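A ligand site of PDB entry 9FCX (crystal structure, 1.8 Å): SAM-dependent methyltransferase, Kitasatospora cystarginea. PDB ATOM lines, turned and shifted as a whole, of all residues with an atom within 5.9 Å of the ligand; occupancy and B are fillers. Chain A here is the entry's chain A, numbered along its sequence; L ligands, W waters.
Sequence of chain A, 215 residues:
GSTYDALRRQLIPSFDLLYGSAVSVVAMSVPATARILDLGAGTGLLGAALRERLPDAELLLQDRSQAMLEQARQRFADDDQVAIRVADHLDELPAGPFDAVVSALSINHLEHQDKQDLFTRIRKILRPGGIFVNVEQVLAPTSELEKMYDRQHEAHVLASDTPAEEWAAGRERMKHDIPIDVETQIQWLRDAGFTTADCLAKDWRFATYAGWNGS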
ATOM      1  N   TYR A   4      -1.355  -0.194   8.342  1.00  0.00           N
ATOM      2  CA  TYR A   4      -0.078  -0.699   8.908  1.00  0.00           C
ATOM      3  C   TYR A   4      -0.023  -2.223   8.777  1.00  0.00           C
ATOM      4  O   TYR A   4       0.966  -2.741   8.233  1.00  0.00           O
ATOM      5  CB  TYR A   4       0.101  -0.276  10.378  1.00  0.00           C
ATOM      6  CG  TYR A   4       1.359  -0.828  10.996  1.00  0.00           C
ATOM      7  CD1 TYR A   4       2.580  -0.206  10.822  1.00  0.00           C
ATOM      8  CD2 TYR A   4       1.334  -2.003  11.744  1.00  0.00           C
ATOM      9  CE1 TYR A   4       3.743  -0.720  11.373  1.00  0.00           C
ATOM     10  CE2 TYR A   4       2.489  -2.531  12.299  1.00  0.00           C
ATOM     11  CZ  TYR A   4       3.697  -1.881  12.122  1.00  0.00           C
ATOM     12  OH  TYR A   4       4.841  -2.395  12.663  1.00  0.00           O
ATOM     13  N   ARG A   8       2.423  -4.645   6.530  1.00  0.00           N
ATOM     14  CA  ARG A   8       3.283  -5.712   7.111  1.00  0.00           C
ATOM     15  C   ARG A   8       3.113  -6.989   6.265  1.00  0.00           C
ATOM     16  O   ARG A   8       4.138  -7.657   6.005  1.00  0.00           O
ATOM     17  CB  ARG A   8       2.977  -5.916   8.596  1.00  0.00           C
ATOM     18  CG  ARG A   8       3.273  -4.713   9.465  1.00  0.00           C
ATOM     19  CD  ARG A   8       4.670  -4.142   9.297  1.00  0.00           C
ATOM     20  NE  ARG A   8       5.702  -5.043   9.786  1.00  0.00           N
ATOM     21  CZ  ARG A   8       7.017  -4.846   9.676  1.00  0.00           C
ATOM     22  NH1 ARG A   8       7.480  -3.766   9.068  1.00  0.00           N
ATOM     23  NH2 ARG A   8       7.856  -5.733  10.177  1.00  0.00           N
ATOM     24  N   TYR A  19       2.925 -16.103  10.970  1.00  0.00           N
ATOM     25  CA  TYR A  19       2.264 -15.570  12.191  1.00  0.00           C
ATOM     26  C   TYR A  19       1.161 -16.563  12.619  1.00  0.00           C
ATOM     27  O   TYR A  19       1.024 -16.821  13.823  1.00  0.00           O
ATOM     28  CB  TYR A  19       1.733 -14.157  11.976  1.00  0.00           C
ATOM     29  CG  TYR A  19       2.775 -13.064  12.098  1.00  0.00           C
ATOM     30  CD1 TYR A  19       2.795 -12.205  13.175  1.00  0.00           C
ATOM     31  CD2 TYR A  19       3.741 -12.891  11.117  1.00  0.00           C
ATOM     32  CE1 TYR A  19       3.744 -11.199  13.293  1.00  0.00           C
ATOM     33  CE2 TYR A  19       4.695 -11.896  11.214  1.00  0.00           C
ATOM     34  CZ  TYR A  19       4.698 -11.043  12.304  1.00  0.00           C
ATOM     35  OH  TYR A  19       5.636 -10.066  12.401  1.00  0.00           O
ATOM     36  N   ASP A  38       5.389 -11.351  25.326  1.00  0.00           N
ATOM     37  CA  ASP A  38       5.587 -10.946  23.911  1.00  0.00           C
ATOM     38  C   ASP A  38       6.800 -10.002  23.876  1.00  0.00           C
ATOM     39  O   ASP A  38       6.647  -8.817  24.231  1.00  0.00           O
ATOM     40  CB  ASP A  38       4.307 -10.318  23.370  1.00  0.00           C
ATOM     41  CG  ASP A  38       4.286  -9.998  21.885  1.00  0.00           C
ATOM     42  OD1 ASP A  38       5.329 -10.207  21.216  1.00  0.00           O
ATOM     43  OD2 ASP A  38       3.227  -9.537  21.418  1.00  0.00           O
ATOM     44  N   LEU A  39       7.971 -10.531  23.484  1.00  0.00           N
ATOM     45  CA  LEU A  39       9.270  -9.788  23.480  1.00  0.00           C
ATOM     46  C   LEU A  39       9.404  -9.001  22.183  1.00  0.00           C
ATOM     47  O   LEU A  39       9.242  -9.615  21.108  1.00  0.00           O
ATOM     48  CB  LEU A  39      10.432 -10.780  23.616  1.00  0.00           C
ATOM     49  CG  LEU A  39      10.533 -11.534  24.940  1.00  0.00           C
ATOM     50  CD1 LEU A  39      11.683 -12.519  24.899  1.00  0.00           C
ATOM     51  CD2 LEU A  39      10.690 -10.580  26.112  1.00  0.00           C
ATOM     52  N   GLY A  40       9.722  -7.709  22.277  1.00  0.00           N
ATOM     53  CA  GLY A  40       9.800  -6.788  21.126  1.00  0.00           C
ATOM     54  C   GLY A  40       8.471  -6.743  20.406  1.00  0.00           C
ATOM     55  O   GLY A  40       8.447  -6.894  19.167  1.00  0.00           O
ATOM     56  N   ALA A  41       7.389  -6.541  21.168  1.00  0.00           N
ATOM     57  CA  ALA A  41       5.978  -6.644  20.738  1.00  0.00           C
ATOM     58  C   ALA A  41       5.677  -5.638  19.614  1.00  0.00           C
ATOM     59  O   ALA A  41       4.731  -5.910  18.851  1.00  0.00           O
ATOM     60  CB  ALA A  41       5.061  -6.430  21.920  1.00  0.00           C
ATOM     61  N   GLY A  42       6.425  -4.535  19.536  1.00  0.00           N
ATOM     62  CA  GLY A  42       6.166  -3.435  18.583  1.00  0.00           C
ATOM     63  C   GLY A  42       4.748  -2.913  18.730  1.00  0.00           C
ATOM     64  O   GLY A  42       4.368  -2.592  19.879  1.00  0.00           O
ATOM     65  N   THR A  43       3.971  -2.902  17.648  1.00  0.00           N
ATOM     66  CA  THR A  43       2.544  -2.479  17.641  1.00  0.00           C
ATOM     67  C   THR A  43       1.644  -3.599  18.183  1.00  0.00           C
ATOM     68  O   THR A  43       0.428  -3.366  18.287  1.00  0.00           O
ATOM     69  CB  THR A  43       2.070  -2.068  16.236  1.00  0.00           C
ATOM     70  OG1 THR A  43       1.949  -3.250  15.440  1.00  0.00           O
ATOM     71  CG2 THR A  43       2.985  -1.067  15.561  1.00  0.00           C
ATOM     72  N   GLY A  44       2.199  -4.780  18.497  1.00  0.00           N
ATOM     73  CA  GLY A  44       1.470  -5.914  19.105  1.00  0.00           C
ATOM     74  C   GLY A  44       0.744  -6.748  18.057  1.00  0.00           C
ATOM     75  O   GLY A  44      -0.340  -7.281  18.372  1.00  0.00           O
ATOM     76  N   LEU A  45       1.333  -6.890  16.870  1.00  0.00           N
ATOM     77  CA  LEU A  45       0.707  -7.569  15.712  1.00  0.00           C
ATOM     78  C   LEU A  45       0.537  -9.068  16.023  1.00  0.00           C
ATOM     79  O   LEU A  45      -0.588  -9.578  15.829  1.00  0.00           O
ATOM     80  CB  LEU A  45       1.574  -7.326  14.471  1.00  0.00           C
ATOM     81  CG  LEU A  45       0.998  -7.782  13.140  1.00  0.00           C
ATOM     82  CD1 LEU A  45      -0.448  -7.308  12.971  1.00  0.00           C
ATOM     83  CD2 LEU A  45       1.857  -7.289  11.996  1.00  0.00           C
ATOM     84  N   LEU A  46       1.588  -9.741  16.494  1.00  0.00           N
ATOM     85  CA  LEU A  46       1.507 -11.181  16.882  1.00  0.00           C
ATOM     86  C   LEU A  46       0.555 -11.312  18.081  1.00  0.00           C
ATOM     87  O   LEU A  46      -0.235 -12.264  18.099  1.00  0.00           O
ATOM     88  CB  LEU A  46       2.894 -11.728  17.216  1.00  0.00           C
ATOM     89  CG  LEU A  46       2.930 -13.200  17.628  1.00  0.00           C
ATOM     90  CD1 LEU A  46       2.248 -14.089  16.596  1.00  0.00           C
ATOM     91  CD2 LEU A  46       4.358 -13.673  17.868  1.00  0.00           C
ATOM     92  N   GLN A  62       6.224  -6.327  25.805  1.00  0.00           N
ATOM     93  CA  GLN A  62       7.384  -5.475  26.152  1.00  0.00           C
ATOM     94  C   GLN A  62       8.234  -5.183  24.920  1.00  0.00           C
ATOM     95  O   GLN A  62       8.242  -5.994  23.967  1.00  0.00           O
ATOM     96  CB  GLN A  62       8.176  -6.042  27.330  1.00  0.00           C
ATOM     97  CG  GLN A  62       8.985  -7.299  27.029  1.00  0.00           C
ATOM     98  CD  GLN A  62       9.902  -7.580  28.196  1.00  0.00           C
ATOM     99  OE1 GLN A  62       9.464  -7.638  29.346  1.00  0.00           O
ATOM    100  NE2 GLN A  62      11.186  -7.714  27.913  1.00  0.00           N
ATOM    101  N   ASP A  63       8.905  -4.037  24.955  1.00  0.00           N
ATOM    102  CA  ASP A  63       9.691  -3.451  23.851  1.00  0.00           C
ATOM    103  C   ASP A  63      10.575  -2.354  24.448  1.00  0.00           C
ATOM    104  O   ASP A  63      10.200  -1.800  25.493  1.00  0.00           O
ATOM    105  CB  ASP A  63       8.771  -2.909  22.761  1.00  0.00           C
ATOM    106  CG  ASP A  63       9.415  -2.849  21.391  1.00  0.00           C
ATOM    107  OD1 ASP A  63       9.036  -3.668  20.539  1.00  0.00           O
ATOM    108  OD2 ASP A  63      10.291  -1.977  21.192  1.00  0.00           O
ATOM    109  N   ARG A  64      11.710  -2.066  23.810  1.00  0.00           N
ATOM    110  CA  ARG A  64      12.622  -0.975  24.238  1.00  0.00           C
ATOM    111  C   ARG A  64      12.019   0.371  23.818  1.00  0.00           C
ATOM    112  O   ARG A  64      12.370   1.384  24.440  1.00  0.00           O
ATOM    113  CB  ARG A  64      14.032  -1.184  23.660  1.00  0.00           C
ATOM    114  CG  ARG A  64      14.140  -1.018  22.156  1.00  0.00           C
ATOM    115  CD  ARG A  64      15.568  -1.132  21.656  1.00  0.00           C
ATOM    116  NE  ARG A  64      15.641  -1.075  20.199  1.00  0.00           N
ATOM    117  CZ  ARG A  64      16.714  -1.345  19.469  1.00  0.00           C
ATOM    118  NH1 ARG A  64      17.842  -1.718  20.041  1.00  0.00           N
ATOM    119  NH2 ARG A  64      16.651  -1.257  18.149  1.00  0.00           N
ATOM    120  N   SER A  65      11.126   0.384  22.823  1.00  0.00           N
ATOM    121  CA  SER A  65      10.567   1.604  22.181  1.00  0.00           C
ATOM    122  C   SER A  65       9.199   1.956  22.778  1.00  0.00           C
ATOM    123  O   SER A  65       8.237   1.204  22.525  1.00  0.00           O
ATOM    124  CB  SER A  65      10.473   1.437  20.687  1.00  0.00           C
ATOM    125  OG  SER A  65       9.781   2.514  20.094  1.00  0.00           O
ATOM    126  N   MET A  68       6.740   2.579  19.790  1.00  0.00           N
ATOM    127  CA  MET A  68       6.160   1.318  19.254  1.00  0.00           C
ATOM    128  C   MET A  68       5.060   0.816  20.213  1.00  0.00           C
ATOM    129  O   MET A  68       3.970   0.487  19.719  1.00  0.00           O
ATOM    130  CB  MET A  68       7.230   0.237  19.068  1.00  0.00           C
ATOM    131  CG  MET A  68       8.231   0.556  17.965  1.00  0.00           C
ATOM    132  SD  MET A  68       7.468   0.742  16.321  1.00  0.00           S
ATOM    133  CE  MET A  68       6.889  -0.922  16.029  1.00  0.00           C
ATOM    134  N   ALA A  87      10.963  -2.390  28.258  1.00  0.00           N
ATOM    135  CA  ALA A  87      12.129  -3.221  28.633  1.00  0.00           C
ATOM    136  C   ALA A  87      12.861  -3.681  27.379  1.00  0.00           C
ATOM    137  O   ALA A  87      12.202  -4.174  26.432  1.00  0.00           O
ATOM    138  CB  ALA A  87      11.676  -4.391  29.473  1.00  0.00           C
ATOM    139  N   ASP A  88      14.193  -3.519  27.376  1.00  0.00           N
ATOM    140  CA  ASP A  88      15.094  -4.128  26.375  1.00  0.00           C
ATOM    141  C   ASP A  88      15.128  -5.630  26.623  1.00  0.00           C
ATOM    142  O   ASP A  88      14.962  -6.037  27.792  1.00  0.00           O
ATOM    143  CB  ASP A  88      16.490  -3.497  26.454  1.00  0.00           C
ATOM    144  CG  ASP A  88      17.325  -3.732  25.215  1.00  0.00           C
ATOM    145  OD1 ASP A  88      17.731  -4.887  24.987  1.00  0.00           O
ATOM    146  OD2 ASP A  88      17.544  -2.745  24.478  1.00  0.00           O
ATOM    147  N   HIS A  89      15.347  -6.433  25.566  1.00  0.00           N
ATOM    148  CA  HIS A  89      15.607  -7.892  25.677  1.00  0.00           C
ATOM    149  C   HIS A  89      16.708  -8.137  26.718  1.00  0.00           C
ATOM    150  O   HIS A  89      16.630  -9.151  27.435  1.00  0.00           O
ATOM    151  CB  HIS A  89      16.023  -8.505  24.338  1.00  0.00           C
ATOM    152  CG  HIS A  89      15.054  -8.308  23.224  1.00  0.00           C
ATOM    153  ND1 HIS A  89      13.690  -8.242  23.422  1.00  0.00           N
ATOM    154  CD2 HIS A  89      15.254  -8.192  21.887  1.00  0.00           C
ATOM    155  CE1 HIS A  89      13.093  -8.070  22.262  1.00  0.00           C
ATOM    156  NE2 HIS A  89      14.030  -8.039  21.304  1.00  0.00           N
ATOM    157  N   LEU A  90      17.693  -7.229  26.797  1.00  0.00           N
ATOM    158  CA  LEU A  90      18.903  -7.345  27.650  1.00  0.00           C
ATOM    159  C   LEU A  90      18.597  -6.978  29.106  1.00  0.00           C
ATOM    160  O   LEU A  90      19.411  -7.339  29.981  1.00  0.00           O
ATOM    161  CB  LEU A  90      20.003  -6.436  27.085  1.00  0.00           C
ATOM    162  CG  LEU A  90      20.463  -6.763  25.658  1.00  0.00           C
ATOM    163  CD1 LEU A  90      21.495  -5.752  25.183  1.00  0.00           C
ATOM    164  CD2 LEU A  90      21.017  -8.176  25.578  1.00  0.00           C
ATOM    165  N   SER A 103       7.897 -14.002  20.200  1.00  0.00           N
ATOM    166  CA  SER A 103       8.599 -12.845  19.615  1.00  0.00           C
ATOM    167  C   SER A 103       8.449 -12.919  18.092  1.00  0.00           C
ATOM    168  O   SER A 103       8.420 -14.040  17.558  1.00  0.00           O
ATOM    169  CB  SER A 103      10.044 -12.826  20.041  1.00  0.00           C
ATOM    170  OG  SER A 103      10.645 -11.582  19.744  1.00  0.00           O
ATOM    171  N   ALA A 104       8.325 -11.767  17.444  1.00  0.00           N
ATOM    172  CA  ALA A 104       8.256 -11.656  15.964  1.00  0.00           C
ATOM    173  C   ALA A 104       9.192 -10.544  15.497  1.00  0.00           C
ATOM    174  O   ALA A 104       8.986  -9.387  15.923  1.00  0.00           O
ATOM    175  CB  ALA A 104       6.834 -11.434  15.525  1.00  0.00           C
ATOM    176  N   LEU A 105      10.185 -10.904  14.679  1.00  0.00           N
ATOM    177  CA  LEU A 105      11.070  -9.994  13.897  1.00  0.00           C
ATOM    178  C   LEU A 105      11.811  -9.024  14.823  1.00  0.00           C
ATOM    179  O   LEU A 105      12.011  -7.864  14.417  1.00  0.00           O
ATOM    180  CB  LEU A 105      10.217  -9.238  12.871  1.00  0.00           C
ATOM    181  CG  LEU A 105       9.343 -10.090  11.958  1.00  0.00           C
ATOM    182  CD1 LEU A 105       8.663  -9.225  10.911  1.00  0.00           C
ATOM    183  CD2 LEU A 105      10.142 -11.195  11.283  1.00  0.00           C
ATOM    184  N   SER A 106      12.234  -9.472  16.004  1.00  0.00           N
ATOM    185  CA  SER A 106      12.809  -8.597  17.057  1.00  0.00           C
ATOM    186  C   SER A 106      14.169  -9.117  17.540  1.00  0.00           C
ATOM    187  O   SER A 106      15.093  -8.285  17.680  1.00  0.00           O
ATOM    188  CB  SER A 106      11.842  -8.433  18.194  1.00  0.00           C
ATOM    189  OG  SER A 106      12.334  -7.466  19.113  1.00  0.00           O
ATOM    190  N   HIS A 109      17.858  -8.468  16.194  1.00  0.00           N
ATOM    191  CA  HIS A 109      18.523  -7.172  16.495  1.00  0.00           C
ATOM    192  C   HIS A 109      19.644  -7.353  17.532  1.00  0.00           C
ATOM    193  O   HIS A 109      20.469  -6.423  17.666  1.00  0.00           O
ATOM    194  CB  HIS A 109      17.506  -6.126  16.944  1.00  0.00           C
ATOM    195  CG  HIS A 109      16.550  -5.721  15.863  1.00  0.00           C
ATOM    196  ND1 HIS A 109      16.619  -4.489  15.248  1.00  0.00           N
ATOM    197  CD2 HIS A 109      15.516  -6.374  15.301  1.00  0.00           C
ATOM    198  CE1 HIS A 109      15.667  -4.406  14.334  1.00  0.00           C
ATOM    199  NE2 HIS A 109      14.981  -5.554  14.348  1.00  0.00           N
ATOM    200  N   LEU A 110      19.682  -8.481  18.239  1.00  0.00           N
ATOM    201  CA  LEU A 110      20.706  -8.772  19.279  1.00  0.00           C
ATOM    202  C   LEU A 110      21.956  -9.371  18.624  1.00  0.00           C
ATOM    203  O   LEU A 110      21.812 -10.081  17.603  1.00  0.00           O
ATOM    204  CB  LEU A 110      20.124  -9.747  20.316  1.00  0.00           C
ATOM    205  CG  LEU A 110      18.922  -9.253  21.109  1.00  0.00           C
ATOM    206  CD1 LEU A 110      18.444 -10.322  22.075  1.00  0.00           C
ATOM    207  CD2 LEU A 110      19.251  -7.972  21.856  1.00  0.00           C
HETATM  208  N1  LIG L   1       6.795  -7.838  16.942  1.00  0.00           N
HETATM  209  C1  LIG L   1       6.287  -6.706  16.100  1.00  0.00           C
HETATM  210  C2  LIG L   1       7.379  -5.668  15.820  1.00  0.00           C
HETATM  211  C3  LIG L   1       8.547  -6.171  14.985  1.00  0.00           C
HETATM  212  S1  LIG L   1       9.728  -4.866  14.559  1.00  0.00           S
HETATM  213  C4  LIG L   1       5.755  -7.261  14.780  1.00  0.00           C
HETATM  214  O1  LIG L   1       5.170  -6.523  13.984  1.00  0.00           O
HETATM  215  O2  LIG L   1       5.896  -8.444  14.487  1.00  0.00           O
HETATM  216  C5  LIG L   1      11.034  -5.097  15.779  1.00  0.00           C
HETATM  217  C6  LIG L   1      10.678  -4.638  17.174  1.00  0.00           C
HETATM  218  O3  LIG L   1      11.711  -5.071  18.087  1.00  0.00           O
HETATM  219  C7  LIG L   1      10.551  -3.120  17.346  1.00  0.00           C
HETATM  220  O4  LIG L   1       9.350  -2.793  18.027  1.00  0.00           O
HETATM  221  C8  LIG L   1      11.800  -2.749  18.157  1.00  0.00           C
HETATM  222  O5  LIG L   1      11.594  -1.615  18.967  1.00  0.00           O
HETATM  223  C9  LIG L   1      11.996  -4.014  18.976  1.00  0.00           C
HETATM  224  N2  LIG L   1      13.347  -4.215  19.495  1.00  0.00           N
HETATM  225  C10 LIG L   1      14.515  -4.198  18.761  1.00  0.00           C
HETATM  226  N3  LIG L   1      15.575  -4.420  19.487  1.00  0.00           N
HETATM  227  C11 LIG L   1      15.093  -4.593  20.769  1.00  0.00           C
HETATM  228  C12 LIG L   1      15.736  -4.859  21.998  1.00  0.00           C
HETATM  229  N4  LIG L   1      17.046  -5.001  22.127  1.00  0.00           N
HETATM  230  N5  LIG L   1      14.945  -4.972  23.102  1.00  0.00           N
HETATM  231  C13 LIG L   1      13.623  -4.825  22.968  1.00  0.00           C
HETATM  232  N6  LIG L   1      12.915  -4.575  21.862  1.00  0.00           N
HETATM  233  C14 LIG L   1      13.716  -4.465  20.785  1.00  0.00           C
HETATM  234  O   HOH W   1      13.694  -2.338  15.261  1.00  0.00           O
HETATM  235  O   HOH W   2      19.110  -2.665  22.402  1.00  0.00           O
HETATM  236  O   HOH W   3       4.365  -4.078  14.826  1.00  0.00           O
HETATM  237  O   HOH W   4      13.665   0.242  18.877  1.00  0.00           O
HETATM  238  O   HOH W   5       5.479  -7.350  11.469  1.00  0.00           O
HETATM  239  O   HOH W   6       7.210  -9.670  19.194  1.00  0.00           O
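The side-chain carboxylate (OD2) of Asp 63 sits at hydrogen-bond distance from an oxygen (O5) of the ligand, 2.6 Å away. The side-chain hydroxyl of Tyr 19 is in hydrogen-bond range of an oxygen (O2) of the ligand (2.7 Å). OG of Ser 106 sits at hydrogen-bond distance from O3 of the ligand (2.7 Å). The backbone carbonyl oxygen (O) of Ala 104 sits at hydrogen-bond distance from a nitrogen (N1) of the ligand (2.9 Å). N5 of the ligand is in hydrogen-bond range of N of His 89. The backbone carbonyl oxygen of Gly 40 sits at hydrogen-bond distance from a nitrogen (N1) of the ligand (2.9 Å). OD1 of Asp 88 is in hydrogen-bond range of N4 of the ligand, 2.9 Å away. A nitrogen (N1) of the ligand lies close to the backbone carbonyl oxygen (O) of Ala 41 (3.4 Å). A nitrogen (N6) of the ligand is in hydrogen-bond range of the backbone NH (N) of Arg 64 (3.4 Å). N3 of the ligand lies close to NE of Arg 64 (3.4 Å).
The side-chain carboxylate of Asp 63 is in hydrogen-bond range of the backbone NH of Ala 41, 3.4 Å away. The side-chain carboxylate (OD1) of Asp 63 sits at hydrogen-bond distance from the backbone NH (N) of Gly 42 (2.9 Å). The side-chain carboxylate (OD2) of Asp 63 lies within hydrogen-bond range of the backbone NH (N) of Ser 65 (3.0 Å). The backbone carbonyl oxygen (O) of Asp 63 is in hydrogen-bond range of the backbone NH (N) of Ala 87, 2.9 Å away. N of Gly 40 lies within hydrogen-bond range of O of Gln 62, 2.8 Å away. The backbone NH of Leu 90 is in hydrogen-bond range of the side-chain carboxylate of Asp 88 (3.0 Å). The backbone NH (N) of Ala 41 is in hydrogen-bond range of the backbone carbonyl oxygen (O) of Gln 62, 3.0 Å away. N of Met 68 sits at hydrogen-bond distance from OG of Ser 65 (3.1 Å).
The backbone carbonyl oxygen (O) of Leu 105 lies close to a sulfur (S1) of the ligand (3.8 Å). Gly 42 touches the ligand (CA to O4, 3.3 Å). Leu 45 touches the ligand (CB to O1, 3.7 Å). Ser 65 touches the ligand (CB to O5, 3.7 Å). Met 68 touches the ligand. Ala 87 touches the ligand (O to C13, 3.8 Å). His 109 touches the ligand. Leu 110 touches the ligand. Hydrophobic or aromatic side chains within 4 Å of the ligand: Tyr 19, Leu 45, Met 68, His 89, Ala 104, His 109 and Leu 110. Of the 27 residues printed, 17 come within 4 Å of the ligand.
Water W5 lies within hydrogen-bond range of an oxygen (O1) of the ligand, the guanidinium group of Arg 8 and the side-chain hydroxyl of Tyr 19. Water W3 lies within hydrogen-bond range of the side-chain hydroxyl of Thr 43 (2.6 Å), an oxygen (O1) of the ligand (2.7 Å) and the side-chain hydroxyl of Tyr 4 (2.8 Å). Water W4 lies within hydrogen-bond range of the guanidinium group of Arg 64 (2.7 Å) and an oxygen (O5) of the ligand (2.8 Å). Water W2 lies within hydrogen-bond range of the side-chain carboxylate of Asp 88, the guanidinium group of Arg 64 and a nitrogen (N4) of the ligand.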
